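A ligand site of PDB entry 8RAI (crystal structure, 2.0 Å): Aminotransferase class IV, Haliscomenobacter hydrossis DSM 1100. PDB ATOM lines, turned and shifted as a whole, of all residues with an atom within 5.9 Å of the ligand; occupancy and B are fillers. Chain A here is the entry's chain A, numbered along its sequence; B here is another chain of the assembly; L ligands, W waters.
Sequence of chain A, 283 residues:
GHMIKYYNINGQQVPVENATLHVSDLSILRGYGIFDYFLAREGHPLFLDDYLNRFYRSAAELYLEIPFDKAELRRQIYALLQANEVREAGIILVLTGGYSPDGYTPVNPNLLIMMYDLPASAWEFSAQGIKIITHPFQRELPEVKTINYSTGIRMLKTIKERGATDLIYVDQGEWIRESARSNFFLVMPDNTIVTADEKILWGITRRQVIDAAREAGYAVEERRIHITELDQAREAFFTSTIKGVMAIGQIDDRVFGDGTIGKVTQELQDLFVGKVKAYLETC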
ATOM      1  N   PHE A  35     -16.149  -1.921  -4.008  1.00  0.00           N
ATOM      2  CA  PHE A  35     -15.789  -2.125  -5.430  1.00  0.00           C
ATOM      3  C   PHE A  35     -14.962  -0.936  -5.914  1.00  0.00           C
ATOM      4  O   PHE A  35     -14.840   0.103  -5.227  1.00  0.00           O
ATOM      5  CB  PHE A  35     -17.050  -2.374  -6.249  1.00  0.00           C
ATOM      6  CG  PHE A  35     -17.712  -1.118  -6.667  1.00  0.00           C
ATOM      7  CD1 PHE A  35     -17.651  -0.695  -7.980  1.00  0.00           C
ATOM      8  CD2 PHE A  35     -18.333  -0.324  -5.718  1.00  0.00           C
ATOM      9  CE1 PHE A  35     -18.235   0.488  -8.374  1.00  0.00           C
ATOM     10  CE2 PHE A  35     -18.910   0.882  -6.111  1.00  0.00           C
ATOM     11  CZ  PHE A  35     -18.846   1.288  -7.434  1.00  0.00           C
ATOM     12  N   ASP A  36     -14.438  -1.121  -7.105  1.00  0.00           N
ATOM     13  CA  ASP A  36     -13.772  -0.043  -7.861  1.00  0.00           C
ATOM     14  C   ASP A  36     -14.024  -0.339  -9.344  1.00  0.00           C
ATOM     15  O   ASP A  36     -14.446  -1.464  -9.723  1.00  0.00           O
ATOM     16  CB  ASP A  36     -12.344   0.123  -7.348  1.00  0.00           C
ATOM     17  CG  ASP A  36     -12.010   1.612  -7.186  1.00  0.00           C
ATOM     18  OD1 ASP A  36     -12.370   2.369  -8.124  1.00  0.00           O
ATOM     19  OD2 ASP A  36     -11.508   1.998  -6.111  1.00  0.00           O
ATOM     20  N   TYR A  37     -13.877   0.702 -10.156  1.00  0.00           N
ATOM     21  CA  TYR A  37     -14.152   0.685 -11.608  1.00  0.00           C
ATOM     22  C   TYR A  37     -13.173   1.648 -12.270  1.00  0.00           C
ATOM     23  O   TYR A  37     -13.010   2.804 -11.760  1.00  0.00           O
ATOM     24  CB  TYR A  37     -15.585   1.098 -11.879  1.00  0.00           C
ATOM     25  CG  TYR A  37     -15.871   1.171 -13.350  1.00  0.00           C
ATOM     26  CD1 TYR A  37     -15.693   2.355 -14.038  1.00  0.00           C
ATOM     27  CD2 TYR A  37     -16.307   0.069 -14.059  1.00  0.00           C
ATOM     28  CE1 TYR A  37     -15.909   2.414 -15.405  1.00  0.00           C
ATOM     29  CE2 TYR A  37     -16.543   0.120 -15.418  1.00  0.00           C
ATOM     30  CZ  TYR A  37     -16.333   1.289 -16.093  1.00  0.00           C
ATOM     31  OH  TYR A  37     -16.553   1.372 -17.423  1.00  0.00           O
ATOM     32  N   TYR A  51      -6.242   3.721  -8.249  1.00  0.00           N
ATOM     33  CA  TYR A  51      -7.448   2.897  -8.072  1.00  0.00           C
ATOM     34  C   TYR A  51      -7.164   1.751  -7.096  1.00  0.00           C
ATOM     35  O   TYR A  51      -8.005   1.528  -6.177  1.00  0.00           O
ATOM     36  CB  TYR A  51      -8.003   2.413  -9.395  1.00  0.00           C
ATOM     37  CG  TYR A  51      -8.611   3.462 -10.275  1.00  0.00           C
ATOM     38  CD1 TYR A  51      -9.900   3.923 -10.043  1.00  0.00           C
ATOM     39  CD2 TYR A  51      -7.920   3.972 -11.371  1.00  0.00           C
ATOM     40  CE1 TYR A  51     -10.496   4.867 -10.856  1.00  0.00           C
ATOM     41  CE2 TYR A  51      -8.507   4.926 -12.178  1.00  0.00           C
ATOM     42  CZ  TYR A  51      -9.794   5.366 -11.948  1.00  0.00           C
ATOM     43  OH  TYR A  51     -10.392   6.317 -12.733  1.00  0.00           O
ATOM     44  N   ARG A  54      -7.023   2.819  -3.519  1.00  0.00           N
ATOM     45  CA  ARG A  54      -8.383   3.133  -2.978  1.00  0.00           C
ATOM     46  C   ARG A  54      -9.130   1.812  -2.673  1.00  0.00           C
ATOM     47  O   ARG A  54      -9.858   1.715  -1.644  1.00  0.00           O
ATOM     48  CB  ARG A  54      -9.095   4.070  -3.950  1.00  0.00           C
ATOM     49  CG  ARG A  54     -10.492   4.464  -3.500  1.00  0.00           C
ATOM     50  CD  ARG A  54     -11.205   5.399  -4.449  1.00  0.00           C
ATOM     51  NE  ARG A  54     -11.620   4.821  -5.716  1.00  0.00           N
ATOM     52  CZ  ARG A  54     -12.195   5.530  -6.682  1.00  0.00           C
ATOM     53  NH1 ARG A  54     -12.413   6.822  -6.504  1.00  0.00           N
ATOM     54  NH2 ARG A  54     -12.554   4.966  -7.817  1.00  0.00           N
ATOM     55  N   ARG A 139     -24.610  10.212   1.508  1.00  0.00           N
ATOM     56  CA  ARG A 139     -24.100   8.822   1.389  1.00  0.00           C
ATOM     57  C   ARG A 139     -23.533   8.361   2.734  1.00  0.00           C
ATOM     58  O   ARG A 139     -22.838   9.146   3.451  1.00  0.00           O
ATOM     59  CB  ARG A 139     -22.985   8.715   0.343  1.00  0.00           C
ATOM     60  CG  ARG A 139     -23.467   8.744  -1.098  1.00  0.00           C
ATOM     61  CD  ARG A 139     -22.277   8.664  -2.052  1.00  0.00           C
ATOM     62  NE  ARG A 139     -21.447   7.481  -1.806  1.00  0.00           N
ATOM     63  CZ  ARG A 139     -20.172   7.440  -1.413  1.00  0.00           C
ATOM     64  NH1 ARG A 139     -19.440   8.529  -1.227  1.00  0.00           N
ATOM     65  NH2 ARG A 139     -19.604   6.258  -1.190  1.00  0.00           N
ATOM     66  N   PRO A 142     -19.085   7.774   3.262  1.00  0.00           N
ATOM     67  CA  PRO A 142     -18.788   8.338   1.937  1.00  0.00           C
ATOM     68  C   PRO A 142     -17.339   8.205   1.424  1.00  0.00           C
ATOM     69  O   PRO A 142     -17.134   8.158   0.221  1.00  0.00           O
ATOM     70  CB  PRO A 142     -19.189   9.815   2.112  1.00  0.00           C
ATOM     71  CG  PRO A 142     -19.149  10.032   3.605  1.00  0.00           C
ATOM     72  CD  PRO A 142     -19.685   8.747   4.183  1.00  0.00           C
ATOM     73  N   LYS A 145     -15.627   3.269  -1.039  1.00  0.00           N
ATOM     74  CA  LYS A 145     -16.398   2.875  -2.245  1.00  0.00           C
ATOM     75  C   LYS A 145     -17.167   1.576  -1.985  1.00  0.00           C
ATOM     76  O   LYS A 145     -16.713   0.484  -2.462  1.00  0.00           O
ATOM     77  CB  LYS A 145     -15.453   2.794  -3.441  1.00  0.00           C
ATOM     78  CG  LYS A 145     -16.115   3.117  -4.767  1.00  0.00           C
ATOM     79  CD  LYS A 145     -15.070   3.433  -5.804  1.00  0.00           C
ATOM     80  CE  LYS A 145     -15.584   3.210  -7.212  1.00  0.00           C
ATOM     81  NZ  LYS A 145     -16.602   4.216  -7.536  1.00  0.00           N
ATOM     82  N   TYR A 149     -25.589   1.496  -3.655  1.00  0.00           N
ATOM     83  CA  TYR A 149     -26.010   2.531  -4.631  1.00  0.00           C
ATOM     84  C   TYR A 149     -27.534   2.636  -4.622  1.00  0.00           C
ATOM     85  O   TYR A 149     -28.036   3.163  -5.636  1.00  0.00           O
ATOM     86  CB  TYR A 149     -25.425   2.290  -6.037  1.00  0.00           C
ATOM     87  CG  TYR A 149     -23.994   2.727  -6.130  1.00  0.00           C
ATOM     88  CD1 TYR A 149     -23.013   1.910  -5.595  1.00  0.00           C
ATOM     89  CD2 TYR A 149     -23.596   3.973  -6.610  1.00  0.00           C
ATOM     90  CE1 TYR A 149     -21.688   2.288  -5.566  1.00  0.00           C
ATOM     91  CE2 TYR A 149     -22.253   4.368  -6.607  1.00  0.00           C
ATOM     92  CZ  TYR A 149     -21.300   3.528  -6.038  1.00  0.00           C
ATOM     93  OH  TYR A 149     -19.968   3.829  -5.973  1.00  0.00           O
ATOM     94  N   GLU A 178     -21.764  15.392  -3.815  1.00  0.00           N
ATOM     95  CA  GLU A 178     -21.381  14.709  -5.059  1.00  0.00           C
ATOM     96  C   GLU A 178     -22.651  14.069  -5.636  1.00  0.00           C
ATOM     97  O   GLU A 178     -23.675  14.068  -4.929  1.00  0.00           O
ATOM     98  CB  GLU A 178     -20.255  13.720  -4.718  1.00  0.00           C
ATOM     99  CG  GLU A 178     -20.731  12.551  -3.859  1.00  0.00           C
ATOM    100  CD  GLU A 178     -19.627  11.706  -3.288  1.00  0.00           C
ATOM    101  OE1 GLU A 178     -18.638  11.491  -3.988  1.00  0.00           O
ATOM    102  OE2 GLU A 178     -19.799  11.228  -2.149  1.00  0.00           O
ATOM    103  N   SER A 179     -22.602  13.558  -6.873  1.00  0.00           N
ATOM    104  CA  SER A 179     -23.674  12.683  -7.395  1.00  0.00           C
ATOM    105  C   SER A 179     -23.403  11.242  -6.925  1.00  0.00           C
ATOM    106  O   SER A 179     -22.466  10.988  -6.110  1.00  0.00           O
ATOM    107  CB  SER A 179     -23.855  12.815  -8.905  1.00  0.00           C
ATOM    108  OG  SER A 179     -23.045  11.902  -9.619  1.00  0.00           O
ATOM    109  N   ALA A 180     -24.272  10.327  -7.329  1.00  0.00           N
ATOM    110  CA  ALA A 180     -24.193   8.899  -6.947  1.00  0.00           C
ATOM    111  C   ALA A 180     -22.892   8.322  -7.506  1.00  0.00           C
ATOM    112  O   ALA A 180     -22.396   7.416  -6.886  1.00  0.00           O
ATOM    113  CB  ALA A 180     -25.402   8.154  -7.448  1.00  0.00           C
ATOM    114  N   ARG A 181     -22.370   8.824  -8.646  1.00  0.00           N
ATOM    115  CA  ARG A 181     -21.253   8.216  -9.398  1.00  0.00           C
ATOM    116  C   ARG A 181     -20.241   9.286  -9.853  1.00  0.00           C
ATOM    117  O   ARG A 181     -19.403   8.940 -10.745  1.00  0.00           O
ATOM    118  CB  ARG A 181     -21.828   7.448 -10.591  1.00  0.00           C
ATOM    119  CG  ARG A 181     -22.694   6.263 -10.206  1.00  0.00           C
ATOM    120  CD  ARG A 181     -22.917   5.315 -11.365  1.00  0.00           C
ATOM    121  NE  ARG A 181     -23.860   5.824 -12.371  1.00  0.00           N
ATOM    122  CZ  ARG A 181     -24.216   5.147 -13.488  1.00  0.00           C
ATOM    123  NH1 ARG A 181     -23.735   3.940 -13.734  1.00  0.00           N
ATOM    124  NH2 ARG A 181     -25.075   5.682 -14.334  1.00  0.00           N
ATOM    125  N   SER A 182     -20.289  10.514  -9.316  1.00  0.00           N
ATOM    126  CA  SER A 182     -19.421  11.625  -9.835  1.00  0.00           C
ATOM    127  C   SER A 182     -19.059  12.596  -8.725  1.00  0.00           C
ATOM    128  O   SER A 182     -19.896  12.869  -7.908  1.00  0.00           O
ATOM    129  CB  SER A 182     -20.098  12.379 -10.967  1.00  0.00           C
ATOM    130  OG  SER A 182     -20.413  11.510 -12.021  1.00  0.00           O
ATOM    131  N   ASN A 183     -17.882  13.213  -8.787  1.00  0.00           N
ATOM    132  CA  ASN A 183     -17.567  14.386  -7.964  1.00  0.00           C
ATOM    133  C   ASN A 183     -18.111  15.633  -8.667  1.00  0.00           C
ATOM    134  O   ASN A 183     -18.361  15.608  -9.873  1.00  0.00           O
ATOM    135  CB  ASN A 183     -16.072  14.454  -7.611  1.00  0.00           C
ATOM    136  CG  ASN A 183     -15.647  13.319  -6.703  1.00  0.00           C
ATOM    137  OD1 ASN A 183     -14.822  12.465  -7.065  1.00  0.00           O
ATOM    138  ND2 ASN A 183     -16.142  13.345  -5.489  1.00  0.00           N
ATOM    139  N   LEU A 201     -16.641  10.669  -1.666  1.00  0.00           N
ATOM    140  CA  LEU A 201     -15.603   9.753  -2.196  1.00  0.00           C
ATOM    141  C   LEU A 201     -14.512  10.615  -2.816  1.00  0.00           C
ATOM    142  O   LEU A 201     -14.855  11.532  -3.563  1.00  0.00           O
ATOM    143  CB  LEU A 201     -16.190   8.787  -3.225  1.00  0.00           C
ATOM    144  CG  LEU A 201     -15.230   7.653  -3.610  1.00  0.00           C
ATOM    145  CD1 LEU A 201     -15.185   6.624  -2.489  1.00  0.00           C
ATOM    146  CD2 LEU A 201     -15.626   7.016  -4.932  1.00  0.00           C
ATOM    147  N   TRP A 202     -13.265  10.314  -2.521  1.00  0.00           N
ATOM    148  CA  TRP A 202     -12.099  10.973  -3.154  1.00  0.00           C
ATOM    149  C   TRP A 202     -11.838  10.318  -4.515  1.00  0.00           C
ATOM    150  O   TRP A 202     -11.121   9.308  -4.626  1.00  0.00           O
ATOM    151  CB  TRP A 202     -10.900  11.028  -2.189  1.00  0.00           C
ATOM    152  CG  TRP A 202     -10.971  12.214  -1.275  1.00  0.00           C
ATOM    153  CD1 TRP A 202     -12.104  12.843  -0.831  1.00  0.00           C
ATOM    154  CD2 TRP A 202      -9.866  12.970  -0.717  1.00  0.00           C
ATOM    155  NE1 TRP A 202     -11.787  13.913  -0.032  1.00  0.00           N
ATOM    156  CE2 TRP A 202     -10.422  14.023   0.052  1.00  0.00           C
ATOM    157  CE3 TRP A 202      -8.460  12.848  -0.765  1.00  0.00           C
ATOM    158  CZ2 TRP A 202      -9.630  14.939   0.746  1.00  0.00           C
ATOM    159  CZ3 TRP A 202      -7.687  13.752  -0.076  1.00  0.00           C
ATOM    160  CH2 TRP A 202      -8.260  14.782   0.669  1.00  0.00           C
ATOM    161  N   GLY A 203     -12.500  10.844  -5.545  1.00  0.00           N
ATOM    162  CA  GLY A 203     -12.399  10.258  -6.883  1.00  0.00           C
ATOM    163  C   GLY A 203     -10.993  10.326  -7.454  1.00  0.00           C
ATOM    164  O   GLY A 203     -10.258  11.294  -7.176  1.00  0.00           O
ATOM    165  N   ILE A 204     -10.636   9.356  -8.295  1.00  0.00           N
ATOM    166  CA  ILE A 204      -9.337   9.412  -8.994  1.00  0.00           C
ATOM    167  C   ILE A 204      -9.390  10.569  -9.997  1.00  0.00           C
ATOM    168  O   ILE A 204      -8.403  11.281 -10.147  1.00  0.00           O
ATOM    169  CB  ILE A 204      -8.982   8.078  -9.660  1.00  0.00           C
ATOM    170  CG1 ILE A 204      -8.926   6.904  -8.667  1.00  0.00           C
ATOM    171  CG2 ILE A 204      -7.724   8.252 -10.475  1.00  0.00           C
ATOM    172  CD1 ILE A 204      -8.574   7.222  -7.279  1.00  0.00           C
ATOM    173  N   THR A 205     -10.524  10.758 -10.681  1.00  0.00           N
ATOM    174  CA  THR A 205     -10.678  11.830 -11.681  1.00  0.00           C
ATOM    175  C   THR A 205     -10.565  13.206 -11.000  1.00  0.00           C
ATOM    176  O   THR A 205      -9.789  14.072 -11.536  1.00  0.00           O
ATOM    177  CB  THR A 205     -11.935  11.646 -12.532  1.00  0.00           C
ATOM    178  OG1 THR A 205     -12.095  10.252 -12.842  1.00  0.00           O
ATOM    179  CG2 THR A 205     -11.795  12.419 -13.814  1.00  0.00           C
ATOM    180  N   ARG A 206     -11.288  13.390  -9.894  1.00  0.00           N
ATOM    181  CA  ARG A 206     -11.218  14.576  -9.008  1.00  0.00           C
ATOM    182  C   ARG A 206      -9.744  14.900  -8.684  1.00  0.00           C
ATOM    183  O   ARG A 206      -9.304  16.070  -8.876  1.00  0.00           O
ATOM    184  CB  ARG A 206     -12.068  14.270  -7.780  1.00  0.00           C
ATOM    185  CG  ARG A 206     -11.954  15.287  -6.646  1.00  0.00           C
ATOM    186  CD  ARG A 206     -12.614  14.742  -5.399  1.00  0.00           C
ATOM    187  NE  ARG A 206     -12.648  15.754  -4.353  1.00  0.00           N
ATOM    188  CZ  ARG A 206     -11.611  16.119  -3.587  1.00  0.00           C
ATOM    189  NH1 ARG A 206     -10.452  15.537  -3.696  1.00  0.00           N
ATOM    190  NH2 ARG A 206     -11.758  17.089  -2.697  1.00  0.00           N
ATOM    191  N   THR A 239     -16.778  15.248 -12.374  1.00  0.00           N
ATOM    192  CA  THR A 239     -15.648  14.366 -12.717  1.00  0.00           C
ATOM    193  C   THR A 239     -16.068  12.917 -12.395  1.00  0.00           C
ATOM    194  O   THR A 239     -16.704  12.718 -11.368  1.00  0.00           O
ATOM    195  CB  THR A 239     -14.356  14.795 -12.006  1.00  0.00           C
ATOM    196  OG1 THR A 239     -14.554  14.659 -10.619  1.00  0.00           O
ATOM    197  CG2 THR A 239     -13.987  16.241 -12.294  1.00  0.00           C
ATOM    198  N   SER A 240     -15.705  11.975 -13.243  1.00  0.00           N
ATOM    199  CA  SER A 240     -15.783  10.536 -12.919  1.00  0.00           C
ATOM    200  C   SER A 240     -14.916   9.796 -13.905  1.00  0.00           C
ATOM    201  O   SER A 240     -14.566  10.368 -14.964  1.00  0.00           O
ATOM    202  CB  SER A 240     -17.208   9.988 -12.957  1.00  0.00           C
ATOM    203  OG  SER A 240     -17.721   9.905 -14.287  1.00  0.00           O
ATOM    204  N   THR A 241     -14.635   8.543 -13.583  1.00  0.00           N
ATOM    205  CA  THR A 241     -13.882   7.641 -14.472  1.00  0.00           C
ATOM    206  C   THR A 241     -14.463   7.645 -15.888  1.00  0.00           C
ATOM    207  O   THR A 241     -13.678   7.754 -16.822  1.00  0.00           O
ATOM    208  CB  THR A 241     -13.822   6.251 -13.874  1.00  0.00           C
ATOM    209  OG1 THR A 241     -12.985   6.353 -12.730  1.00  0.00           O
ATOM    210  CG2 THR A 241     -13.298   5.268 -14.878  1.00  0.00           C
ATOM    211  N   ILE A 242     -15.782   7.498 -16.040  1.00  0.00           N
ATOM    212  CA  ILE A 242     -16.444   7.408 -17.391  1.00  0.00           C
ATOM    213  C   ILE A 242     -16.614   8.800 -18.018  1.00  0.00           C
ATOM    214  O   ILE A 242     -16.430   8.940 -19.252  1.00  0.00           O
ATOM    215  CB  ILE A 242     -17.784   6.641 -17.348  1.00  0.00           C
ATOM    216  CG1 ILE A 242     -17.519   5.182 -16.992  1.00  0.00           C
ATOM    217  CG2 ILE A 242     -18.521   6.748 -18.678  1.00  0.00           C
ATOM    218  CD1 ILE A 242     -18.775   4.344 -16.741  1.00  0.00           C
ATOM    219  N   ARG B  30     -24.318  -3.416  -6.739  1.00  0.00           N
ATOM    220  CA  ARG B  30     -24.857  -2.092  -6.346  1.00  0.00           C
ATOM    221  C   ARG B  30     -25.668  -2.144  -5.047  1.00  0.00           C
ATOM    222  O   ARG B  30     -26.273  -1.106  -4.673  1.00  0.00           O
ATOM    223  CB  ARG B  30     -25.737  -1.502  -7.458  1.00  0.00           C
ATOM    224  CG  ARG B  30     -25.027  -1.276  -8.783  1.00  0.00           C
ATOM    225  CD  ARG B  30     -23.879  -0.261  -8.758  1.00  0.00           C
ATOM    226  NE  ARG B  30     -23.099  -0.474  -9.963  1.00  0.00           N
ATOM    227  CZ  ARG B  30     -21.876  -1.004 -10.047  1.00  0.00           C
ATOM    228  NH1 ARG B  30     -21.123  -1.282  -8.985  1.00  0.00           N
ATOM    229  NH2 ARG B  30     -21.368  -1.223 -11.243  1.00  0.00           N
ATOM    230  N   GLY B 103     -25.233  -2.404 -15.207  1.00  0.00           N
ATOM    231  CA  GLY B 103     -24.642  -2.398 -13.866  1.00  0.00           C
ATOM    232  C   GLY B 103     -25.217  -1.288 -13.018  1.00  0.00           C
ATOM    233  O   GLY B 103     -24.501  -0.884 -12.090  1.00  0.00           O
ATOM    234  N   TYR B 104     -26.450  -0.855 -13.298  1.00  0.00           N
ATOM    235  CA  TYR B 104     -27.104   0.270 -12.598  1.00  0.00           C
ATOM    236  C   TYR B 104     -28.631   0.265 -12.743  1.00  0.00           C
ATOM    237  O   TYR B 104     -29.270   0.445 -11.734  1.00  0.00           O
ATOM    238  CB  TYR B 104     -26.568   1.628 -13.080  1.00  0.00           C
ATOM    239  CG  TYR B 104     -26.621   2.711 -12.040  1.00  0.00           C
ATOM    240  CD1 TYR B 104     -25.815   2.657 -10.913  1.00  0.00           C
ATOM    241  CD2 TYR B 104     -27.415   3.831 -12.207  1.00  0.00           C
ATOM    242  CE1 TYR B 104     -25.788   3.687  -9.986  1.00  0.00           C
ATOM    243  CE2 TYR B 104     -27.456   4.839 -11.256  1.00  0.00           C
ATOM    244  CZ  TYR B 104     -26.638   4.769 -10.138  1.00  0.00           C
ATOM    245  OH  TYR B 104     -26.666   5.751  -9.201  1.00  0.00           O
HETATM  246  N1  LIG L   1     -18.190   5.706  -9.183  1.00  0.00           N
HETATM  247  C1  LIG L   1     -17.455   9.960  -7.088  1.00  0.00           C
HETATM  248  C2  LIG L   1     -17.100   9.026  -8.035  1.00  0.00           C
HETATM  249  C3  LIG L   1     -17.707   7.762  -8.002  1.00  0.00           C
HETATM  250  C4  LIG L   1     -18.638   7.509  -6.970  1.00  0.00           C
HETATM  251  C5  LIG L   1     -18.941   8.517  -6.041  1.00  0.00           C
HETATM  252  N2  LIG L   1     -18.334   9.693  -6.100  1.00  0.00           N
HETATM  253  C6  LIG L   1     -19.926   8.278  -4.942  1.00  0.00           C
HETATM  254  O1  LIG L   1     -19.253   6.298  -6.850  1.00  0.00           O
HETATM  255  C7  LIG L   1     -17.408   6.719  -8.996  1.00  0.00           C
HETATM  256  C8  LIG L   1     -16.061   9.380  -9.038  1.00  0.00           C
HETATM  257  O2  LIG L   1     -14.850   8.623  -8.720  1.00  0.00           O
HETATM  258  P1  LIG L   1     -13.749   8.320  -9.874  1.00  0.00           P
HETATM  259  O3  LIG L   1     -12.651   7.650  -9.102  1.00  0.00           O
HETATM  260  O4  LIG L   1     -14.460   7.481 -10.952  1.00  0.00           O
HETATM  261  O5  LIG L   1     -13.321   9.681 -10.532  1.00  0.00           O
HETATM  262  N3  LIG L   1     -17.967   4.898 -10.283  1.00  0.00           N
HETATM  263  C9  LIG L   1     -18.933   3.944 -10.682  1.00  0.00           C
HETATM  264  C10 LIG L   1     -18.830   3.327 -11.922  1.00  0.00           C
HETATM  265  C11 LIG L   1     -19.797   2.390 -12.311  1.00  0.00           C
HETATM  266  C12 LIG L   1     -20.857   2.068 -11.473  1.00  0.00           C
HETATM  267  C13 LIG L   1     -20.971   2.702 -10.245  1.00  0.00           C
HETATM  268  C14 LIG L   1     -20.013   3.633  -9.847  1.00  0.00           C
HETATM  269  O   HOH W   1     -22.405   0.428 -14.014  1.00  0.00           O
HETATM  270  O   HOH W   2     -13.855  12.047  -9.628  1.00  0.00           O
HETATM  271  O   HOH W   3     -14.514   4.608 -10.476  1.00  0.00           O
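Water W2 lies within hydrogen-bond range of an oxygen (O5) of the ligand, the side-chain amide oxygen of Asn 183, the side-chain hydroxyl of Thr 239 and the backbone NH of Arg 206. Water W3 lies within hydrogen-bond range of O of Tyr 37 (2.7 Å), O4 of the ligand (2.9 Å), OG1 of Thr 241 (3.2 Å) and NH2 of Arg 54 (3.3 Å). Water W1 lies within hydrogen-bond range of O of Gly 103 of chain B and NH2 of Arg 30 of chain B.
Residues that only touch the ligand: Phe 35 (3.6 Å), Tyr 37 (3.9 Å), Tyr 51 (3.9 Å), Arg 139 (3.6 Å), Ser 179 (3.9 Å), Arg 181 (3.4 Å), Ser 182 (3.5 Å), Asn 183 (3.6 Å), Leu 201 (3.7 Å), Gly 203 (3.4 Å), Ser 240 (3.5 Å) and Arg 30 of chain B (3.3 Å). Hydrophobic or aromatic side chains that line the ligand: Phe 35, Tyr 37, Tyr 51, Tyr 149, Leu 201 and Ile 204. 20 residues have an atom within 4 Å of the ligand: Phe 35, Tyr 37, Tyr 51, Arg 54, Arg 139, Lys 145, Tyr 149, Glu 178, Ser 179, Ala 180, Arg 181, Ser 182, Asn 183, Leu 201, Gly 203, Ile 204, Thr 205, Ser 240, Thr 241 and Arg 30 of chain B. Along chain A the residues within 4 Å of the ligand span positions 35 to 241.
The side-chain hydroxyl (OG1) of Thr 241 lies within hydrogen-bond range of the side-chain hydroxyl (OH) of Tyr 51. The backbone NH (N) of Tyr 149 sits at hydrogen-bond distance from the backbone carbonyl oxygen (O) of Arg 30 of chain B (2.9 Å). The backbone carbonyl oxygen (O) of Lys 145 sits at hydrogen-bond distance from the backbone NH (N) of Phe 35, 2.9 Å away. The guanidinium group of Arg 54 lies within hydrogen-bond range of the backbone carbonyl oxygen of Trp 202 (3.4 Å). The side-chain carboxylate of Glu 178 lies within hydrogen-bond range of the side-chain amide nitrogen of Asn 183 (3.5 Å). The backbone NH (N) of Leu 201 lies within hydrogen-bond range of the side-chain carboxylate (OE1) of Glu 178 (3.2 Å). The side-chain hydroxyl (OG) of Ser 179 is in hydrogen-bond range of the backbone NH (N) of Ser 182. N of Leu 201 is in hydrogen-bond range of O of Pro 142.
The backbone NH (N) of Thr 241 sits at hydrogen-bond distance from an oxygen (O4) of the ligand, at 2.8 Å. OG1 of Thr 241 is in hydrogen-bond range of O4 of the ligand. An oxygen (O5) of the ligand is in hydrogen-bond range of the backbone NH (N) of Thr 205 (3.0 Å). O5 of the ligand sits at hydrogen-bond distance from OG1 of Thr 205 (2.7 Å). An oxygen (O1) of the ligand sits at hydrogen-bond distance from the side-chain hydroxyl of Tyr 149, at 2.7 Å. NZ of Lys 145 is in hydrogen-bond range of N1 of the ligand, at 2.7 Å. The guanidinium group of Arg 54 lies within salt-bridge range of an oxygen (O3) of the ligand (2.7 Å). An oxygen (O3) of the ligand sits at hydrogen-bond distance from the backbone NH of Ile 204. A nitrogen (N2) of the ligand lies within hydrogen-bond range of the side-chain carboxylate (OE1) of Glu 178, 2.8 Å away. O of Ala 180 sits close to O1 of the ligand (3.3 Å).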
